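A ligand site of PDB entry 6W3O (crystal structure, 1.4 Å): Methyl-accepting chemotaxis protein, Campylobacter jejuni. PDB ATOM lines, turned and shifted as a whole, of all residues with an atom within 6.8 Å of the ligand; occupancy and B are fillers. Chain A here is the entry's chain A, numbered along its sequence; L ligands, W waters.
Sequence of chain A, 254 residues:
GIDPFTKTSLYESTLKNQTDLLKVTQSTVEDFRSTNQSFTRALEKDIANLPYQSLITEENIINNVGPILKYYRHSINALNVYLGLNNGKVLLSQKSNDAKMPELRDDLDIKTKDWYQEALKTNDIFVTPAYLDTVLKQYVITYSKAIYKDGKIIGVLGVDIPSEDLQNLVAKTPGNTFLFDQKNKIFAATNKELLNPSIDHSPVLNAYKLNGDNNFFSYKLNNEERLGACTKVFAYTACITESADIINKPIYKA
OD1 of Asp 133 is in salt-bridge range of N1 of the ligand (2.6 Å).
The backbone NH (N) of Thr 134 lies within hydrogen-bond range of an oxygen (O1) of the ligand (3.0 Å).
An oxygen (O1) of the ligand sits at hydrogen-bond distance from the side-chain hydroxyl of Thr 134, at 2.7 Å.
The side-chain carboxylate (OD2) of Asp 160 is in salt-bridge range of a nitrogen (N1) of the ligand (2.7 Å).
OH of Tyr 131 lies within hydrogen-bond range of N1 of the ligand, 2.8 Å away.
The indole nitrogen of Trp 115 is in hydrogen-bond range of an oxygen (O2) of the ligand (2.9 Å).
OD2 of Asp 133 sits at hydrogen-bond distance from N of Val 135 (3.3 Å).
OD2 of Asp 133 sits at hydrogen-bond distance from ND2 of Asn 80 (3.1 Å).
The side-chain carboxylate of Asp 133 lies within hydrogen-bond range of the backbone NH of Leu 136 (2.7 Å).
The side-chain amino group (NZ) of Lys 113 is in hydrogen-bond range of the side-chain hydroxyl (OG1) of Thr 134 (3.4 Å).
The side-chain hydroxyl (OH) of Tyr 82 is in hydrogen-bond range of the side-chain carboxylate (OD1) of Asp 160, 2.7 Å away.
The backbone NH (N) of Asp 160 lies within hydrogen-bond range of the backbone carbonyl oxygen (O) of Asn 80 (2.9 Å).
The side-chain hydroxyl of Tyr 131 is in hydrogen-bond range of the side-chain hydroxyl of Thr 142 (2.6 Å).
The backbone NH (N) of Val 140 sits at hydrogen-bond distance from the backbone carbonyl oxygen (O) of Tyr 131, 2.9 Å away.
Residues that only touch the ligand: Tyr 82 (3.5 Å), Lys 113 (3.5 Å) and Val 135 (3.7 Å).
Hydrophobic or aromatic side chains that line the ligand: Tyr 82, Trp 115, Tyr 131 and Val 135.
Along chain A the residues within 4 Å of the ligand span positions 82 to 160.
Water W1 lies within hydrogen-bond range of NZ of Lys 113 (2.8 Å), O2 of the ligand (2.9 Å) and OG1 of Thr 134 (3.0 Å).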
ATOM      1  N   ASN A  80      30.974  25.578 -24.992  1.00  0.00           N
ATOM      2  CA  ASN A  80      31.085  24.999 -26.335  1.00  0.00           C
ATOM      3  C   ASN A  80      29.864  25.410 -27.110  1.00  0.00           C
ATOM      4  O   ASN A  80      28.748  25.417 -26.545  1.00  0.00           O
ATOM      5  CB  ASN A  80      31.123  23.471 -26.361  1.00  0.00           C
ATOM      6  CG  ASN A  80      32.315  22.882 -25.628  1.00  0.00           C
ATOM      7  OD1 ASN A  80      33.465  23.175 -25.932  1.00  0.00           O
ATOM      8  ND2 ASN A  80      32.020  22.030 -24.646  1.00  0.00           N
ATOM      9  N   TYR A  82      28.377  24.319 -31.145  1.00  0.00           N
ATOM     10  CA  TYR A  82      28.758  23.346 -32.169  1.00  0.00           C
ATOM     11  C   TYR A  82      27.608  22.999 -33.082  1.00  0.00           C
ATOM     12  O   TYR A  82      26.442  23.148 -32.736  1.00  0.00           O
ATOM     13  CB  TYR A  82      29.376  22.079 -31.546  1.00  0.00           C
ATOM     14  CG  TYR A  82      28.637  21.527 -30.343  1.00  0.00           C
ATOM     15  CD1 TYR A  82      28.884  22.031 -29.067  1.00  0.00           C
ATOM     16  CD2 TYR A  82      27.718  20.494 -30.472  1.00  0.00           C
ATOM     17  CE1 TYR A  82      28.223  21.513 -27.957  1.00  0.00           C
ATOM     18  CE2 TYR A  82      27.043  19.975 -29.373  1.00  0.00           C
ATOM     19  CZ  TYR A  82      27.334  20.456 -28.114  1.00  0.00           C
ATOM     20  OH  TYR A  82      26.713  19.939 -27.025  1.00  0.00           O
ATOM     21  N   VAL A  90      31.520  17.056 -36.315  1.00  0.00           N
ATOM     22  CA  VAL A  90      30.959  18.193 -35.580  1.00  0.00           C
ATOM     23  C   VAL A  90      31.891  19.375 -35.682  1.00  0.00           C
ATOM     24  O   VAL A  90      33.111  19.275 -35.409  1.00  0.00           O
ATOM     25  CB  VAL A  90      30.650  17.847 -34.100  1.00  0.00           C
ATOM     26  CG1 VAL A  90      31.894  17.387 -33.341  1.00  0.00           C
ATOM     27  CG2 VAL A  90      30.020  19.022 -33.381  1.00  0.00           C
ATOM     28  N   LEU A  91      31.308  20.508 -36.079  1.00  0.00           N
ATOM     29  CA  LEU A  91      32.050  21.768 -36.069  1.00  0.00           C
ATOM     30  C   LEU A  91      31.981  22.356 -34.669  1.00  0.00           C
ATOM     31  O   LEU A  91      30.880  22.693 -34.193  1.00  0.00           O
ATOM     32  CB  LEU A  91      31.479  22.751 -37.080  1.00  0.00           C
ATOM     33  CG  LEU A  91      32.232  24.087 -37.156  1.00  0.00           C
ATOM     34  CD1 LEU A  91      33.660  23.925 -37.713  1.00  0.00           C
ATOM     35  CD2 LEU A  91      31.450  25.046 -38.024  1.00  0.00           C
ATOM     36  N   LEU A  92      33.124  22.463 -34.014  1.00  0.00           N
ATOM     37  CA  LEU A  92      33.185  22.791 -32.587  1.00  0.00           C
ATOM     38  C   LEU A  92      33.914  24.084 -32.332  1.00  0.00           C
ATOM     39  O   LEU A  92      35.102  24.229 -32.654  1.00  0.00           O
ATOM     40  CB  LEU A  92      33.861  21.637 -31.838  1.00  0.00           C
ATOM     41  CG  LEU A  92      34.154  21.830 -30.352  1.00  0.00           C
ATOM     42  CD1 LEU A  92      32.865  22.084 -29.548  1.00  0.00           C
ATOM     43  CD2 LEU A  92      34.896  20.642 -29.819  1.00  0.00           C
ATOM     44  N   LEU A 108      34.266  12.382 -32.140  1.00  0.00           N
ATOM     45  CA  LEU A 108      33.472  12.644 -30.967  1.00  0.00           C
ATOM     46  C   LEU A 108      32.179  11.819 -30.817  1.00  0.00           C
ATOM     47  O   LEU A 108      31.381  12.070 -29.924  1.00  0.00           O
ATOM     48  CB  LEU A 108      33.251  14.148 -30.828  1.00  0.00           C
ATOM     49  CG  LEU A 108      34.494  14.951 -30.432  1.00  0.00           C
ATOM     50  CD1 LEU A 108      34.231  16.424 -30.474  1.00  0.00           C
ATOM     51  CD2 LEU A 108      35.022  14.583 -29.064  1.00  0.00           C
ATOM     52  N   ASP A 109      31.990  10.836 -31.689  1.00  0.00           N
ATOM     53  CA  ASP A 109      30.916   9.853 -31.548  1.00  0.00           C
ATOM     54  C   ASP A 109      29.560  10.526 -31.347  1.00  0.00           C
ATOM     55  O   ASP A 109      28.785  10.162 -30.457  1.00  0.00           O
ATOM     56  CB  ASP A 109      31.199   8.893 -30.368  1.00  0.00           C
ATOM     57  CG  ASP A 109      32.486   8.117 -30.553  1.00  0.00           C
ATOM     58  OD1 ASP A 109      32.681   7.601 -31.660  1.00  0.00           O
ATOM     59  OD2 ASP A 109      33.315   8.058 -29.615  1.00  0.00           O
ATOM     60  N   ILE A 110      29.253  11.484 -32.197  1.00  0.00           N
ATOM     61  CA  ILE A 110      28.112  12.353 -31.902  1.00  0.00           C
ATOM     62  C   ILE A 110      26.762  11.671 -32.007  1.00  0.00           C
ATOM     63  O   ILE A 110      25.839  12.010 -31.276  1.00  0.00           O
ATOM     64  CB  ILE A 110      28.108  13.673 -32.696  1.00  0.00           C
ATOM     65  CG1 ILE A 110      27.843  13.424 -34.195  1.00  0.00           C
ATOM     66  CG2 ILE A 110      29.374  14.476 -32.413  1.00  0.00           C
ATOM     67  CD1 ILE A 110      27.715  14.683 -35.024  1.00  0.00           C
ATOM     68  N   LYS A 113      25.161  10.407 -28.805  1.00  0.00           N
ATOM     69  CA  LYS A 113      24.859  11.387 -27.767  1.00  0.00           C
ATOM     70  C   LYS A 113      23.360  11.696 -27.686  1.00  0.00           C
ATOM     71  O   LYS A 113      22.703  11.904 -28.692  1.00  0.00           O
ATOM     72  CB  LYS A 113      25.621  12.690 -27.996  1.00  0.00           C
ATOM     73  CG  LYS A 113      27.133  12.549 -28.145  1.00  0.00           C
ATOM     74  CD  LYS A 113      27.795  12.013 -26.890  1.00  0.00           C
ATOM     75  CE  LYS A 113      29.308  12.090 -27.033  1.00  0.00           C
ATOM     76  NZ  LYS A 113      29.947  11.480 -25.854  1.00  0.00           N
ATOM     77  N   TRP A 115      22.064  14.536 -26.748  1.00  0.00           N
ATOM     78  CA  TRP A 115      21.774  15.861 -27.295  1.00  0.00           C
ATOM     79  C   TRP A 115      21.549  15.799 -28.791  1.00  0.00           C
ATOM     80  O   TRP A 115      20.762  16.569 -29.327  1.00  0.00           O
ATOM     81  CB  TRP A 115      22.831  16.899 -26.930  1.00  0.00           C
ATOM     82  CG  TRP A 115      24.229  16.636 -27.445  1.00  0.00           C
ATOM     83  CD1 TRP A 115      25.248  16.148 -26.736  1.00  0.00           C
ATOM     84  CD2 TRP A 115      24.730  16.849 -28.778  1.00  0.00           C
ATOM     85  NE1 TRP A 115      26.374  16.016 -27.517  1.00  0.00           N
ATOM     86  CE2 TRP A 115      26.065  16.395 -28.793  1.00  0.00           C
ATOM     87  CE3 TRP A 115      24.200  17.416 -29.924  1.00  0.00           C
ATOM     88  CZ2 TRP A 115      26.832  16.431 -29.950  1.00  0.00           C
ATOM     89  CZ3 TRP A 115      24.976  17.488 -31.054  1.00  0.00           C
ATOM     90  CH2 TRP A 115      26.270  16.987 -31.058  1.00  0.00           C
ATOM     91  N   TYR A 131      25.727  17.052 -17.248  1.00  0.00           N
ATOM     92  CA  TYR A 131      26.655  15.934 -17.482  1.00  0.00           C
ATOM     93  C   TYR A 131      28.049  16.468 -17.714  1.00  0.00           C
ATOM     94  O   TYR A 131      28.255  17.659 -17.974  1.00  0.00           O
ATOM     95  CB  TYR A 131      26.197  15.043 -18.644  1.00  0.00           C
ATOM     96  CG  TYR A 131      26.290  15.733 -19.965  1.00  0.00           C
ATOM     97  CD1 TYR A 131      25.310  16.625 -20.402  1.00  0.00           C
ATOM     98  CD2 TYR A 131      27.395  15.544 -20.775  1.00  0.00           C
ATOM     99  CE1 TYR A 131      25.443  17.257 -21.619  1.00  0.00           C
ATOM    100  CE2 TYR A 131      27.544  16.190 -21.987  1.00  0.00           C
ATOM    101  CZ  TYR A 131      26.577  17.069 -22.392  1.00  0.00           C
ATOM    102  OH  TYR A 131      26.749  17.767 -23.585  1.00  0.00           O
ATOM    103  N   LEU A 132      29.025  15.569 -17.595  1.00  0.00           N
ATOM    104  CA  LEU A 132      30.408  15.956 -17.748  1.00  0.00           C
ATOM    105  C   LEU A 132      30.807  16.052 -19.209  1.00  0.00           C
ATOM    106  O   LEU A 132      30.809  15.066 -19.937  1.00  0.00           O
ATOM    107  CB  LEU A 132      31.328  14.950 -17.060  1.00  0.00           C
ATOM    108  CG  LEU A 132      32.789  15.369 -16.915  1.00  0.00           C
ATOM    109  CD1 LEU A 132      33.029  16.576 -16.013  1.00  0.00           C
ATOM    110  CD2 LEU A 132      33.634  14.194 -16.403  1.00  0.00           C
ATOM    111  N   ASP A 133      31.122  17.273 -19.647  1.00  0.00           N
ATOM    112  CA  ASP A 133      31.487  17.493 -21.065  1.00  0.00           C
ATOM    113  C   ASP A 133      32.646  16.586 -21.486  1.00  0.00           C
ATOM    114  O   ASP A 133      33.670  16.520 -20.791  1.00  0.00           O
ATOM    115  CB  ASP A 133      31.931  18.943 -21.241  1.00  0.00           C
ATOM    116  CG  ASP A 133      32.271  19.256 -22.654  1.00  0.00           C
ATOM    117  OD1 ASP A 133      31.427  19.082 -23.477  1.00  0.00           O
ATOM    118  OD2 ASP A 133      33.330  19.785 -22.912  1.00  0.00           O
ATOM    119  N   THR A 134      32.538  16.024 -22.674  1.00  0.00           N
ATOM    120  CA  THR A 134      33.552  15.125 -23.215  1.00  0.00           C
ATOM    121  C   THR A 134      34.871  15.841 -23.463  1.00  0.00           C
ATOM    122  O   THR A 134      35.933  15.261 -23.283  1.00  0.00           O
ATOM    123  CB  THR A 134      33.077  14.600 -24.592  1.00  0.00           C
ATOM    124  OG1 THR A 134      31.814  13.937 -24.449  1.00  0.00           O
ATOM    125  CG2 THR A 134      34.080  13.643 -25.171  1.00  0.00           C
ATOM    126  N   VAL A 135      34.810  17.080 -23.955  1.00  0.00           N
ATOM    127  CA  VAL A 135      36.024  17.758 -24.419  1.00  0.00           C
ATOM    128  C   VAL A 135      36.723  18.564 -23.304  1.00  0.00           C
ATOM    129  O   VAL A 135      37.931  18.530 -23.149  1.00  0.00           O
ATOM    130  CB  VAL A 135      35.699  18.629 -25.635  1.00  0.00           C
ATOM    131  CG1 VAL A 135      36.907  19.457 -26.022  1.00  0.00           C
ATOM    132  CG2 VAL A 135      35.309  17.738 -26.803  1.00  0.00           C
ATOM    133  N   LEU A 136      35.957  19.295 -22.535  1.00  0.00           N
ATOM    134  CA  LEU A 136      36.533  20.200 -21.542  1.00  0.00           C
ATOM    135  C   LEU A 136      36.396  19.686 -20.103  1.00  0.00           C
ATOM    136  O   LEU A 136      36.891  20.325 -19.177  1.00  0.00           O
ATOM    137  CB  LEU A 136      35.968  21.619 -21.683  1.00  0.00           C
ATOM    138  CG  LEU A 136      36.419  22.362 -22.969  1.00  0.00           C
ATOM    139  CD1 LEU A 136      35.751  23.712 -23.115  1.00  0.00           C
ATOM    140  CD2 LEU A 136      37.925  22.538 -23.007  1.00  0.00           C
ATOM    141  N   VAL A 140      28.042  20.494 -17.697  1.00  0.00           N
ATOM    142  CA  VAL A 140      27.289  21.387 -18.595  1.00  0.00           C
ATOM    143  C   VAL A 140      25.857  20.955 -18.684  1.00  0.00           C
ATOM    144  O   VAL A 140      25.531  19.775 -18.476  1.00  0.00           O
ATOM    145  CB  VAL A 140      27.893  21.461 -20.003  1.00  0.00           C
ATOM    146  CG1 VAL A 140      29.307  22.045 -19.953  1.00  0.00           C
ATOM    147  CG2 VAL A 140      27.866  20.111 -20.682  1.00  0.00           C
ATOM    148  N   THR A 142      23.237  21.122 -21.836  1.00  0.00           N
ATOM    149  CA  THR A 142      23.264  21.305 -23.262  1.00  0.00           C
ATOM    150  C   THR A 142      21.863  21.616 -23.769  1.00  0.00           C
ATOM    151  O   THR A 142      20.881  20.957 -23.410  1.00  0.00           O
ATOM    152  CB  THR A 142      23.857  20.075 -23.966  1.00  0.00           C
ATOM    153  OG1 THR A 142      25.201  19.910 -23.533  1.00  0.00           O
ATOM    154  CG2 THR A 142      23.777  20.200 -25.506  1.00  0.00           C
ATOM    155  N   ASP A 160      26.576  24.449 -24.939  1.00  0.00           N
ATOM    156  CA  ASP A 160      26.867  23.957 -23.590  1.00  0.00           C
ATOM    157  C   ASP A 160      27.117  25.115 -22.650  1.00  0.00           C
ATOM    158  O   ASP A 160      28.036  25.929 -22.859  1.00  0.00           O
ATOM    159  CB  ASP A 160      28.161  23.097 -23.614  1.00  0.00           C
ATOM    160  CG  ASP A 160      28.066  21.825 -24.423  1.00  0.00           C
ATOM    161  OD1 ASP A 160      26.955  21.416 -24.795  1.00  0.00           O
ATOM    162  OD2 ASP A 160      29.165  21.278 -24.715  1.00  0.00           O
HETATM  163  N1  LIG L   1      29.202  18.536 -24.716  1.00  0.00           N
HETATM  164  C1  LIG L   1      29.142  17.682 -25.910  1.00  0.00           C
HETATM  165  C2  LIG L   1      29.328  16.257 -25.397  1.00  0.00           C
HETATM  166  O1  LIG L   1      30.106  16.025 -24.425  1.00  0.00           O
HETATM  167  C3  LIG L   1      30.207  18.166 -26.933  1.00  0.00           C
HETATM  168  C4  LIG L   1      30.044  17.378 -28.241  1.00  0.00           C
HETATM  169  C5  LIG L   1      30.563  18.270 -29.374  1.00  0.00           C
HETATM  170  C6  LIG L   1      30.823  16.025 -28.175  1.00  0.00           C
HETATM  171  O2  LIG L   1      28.703  15.312 -25.938  1.00  0.00           O
HETATM  172  C7  LIG L   1      31.633  18.214 -26.392  1.00  0.00           C
HETATM  173  O   HOH W   1      28.934  13.212 -23.894  1.00  0.00           O
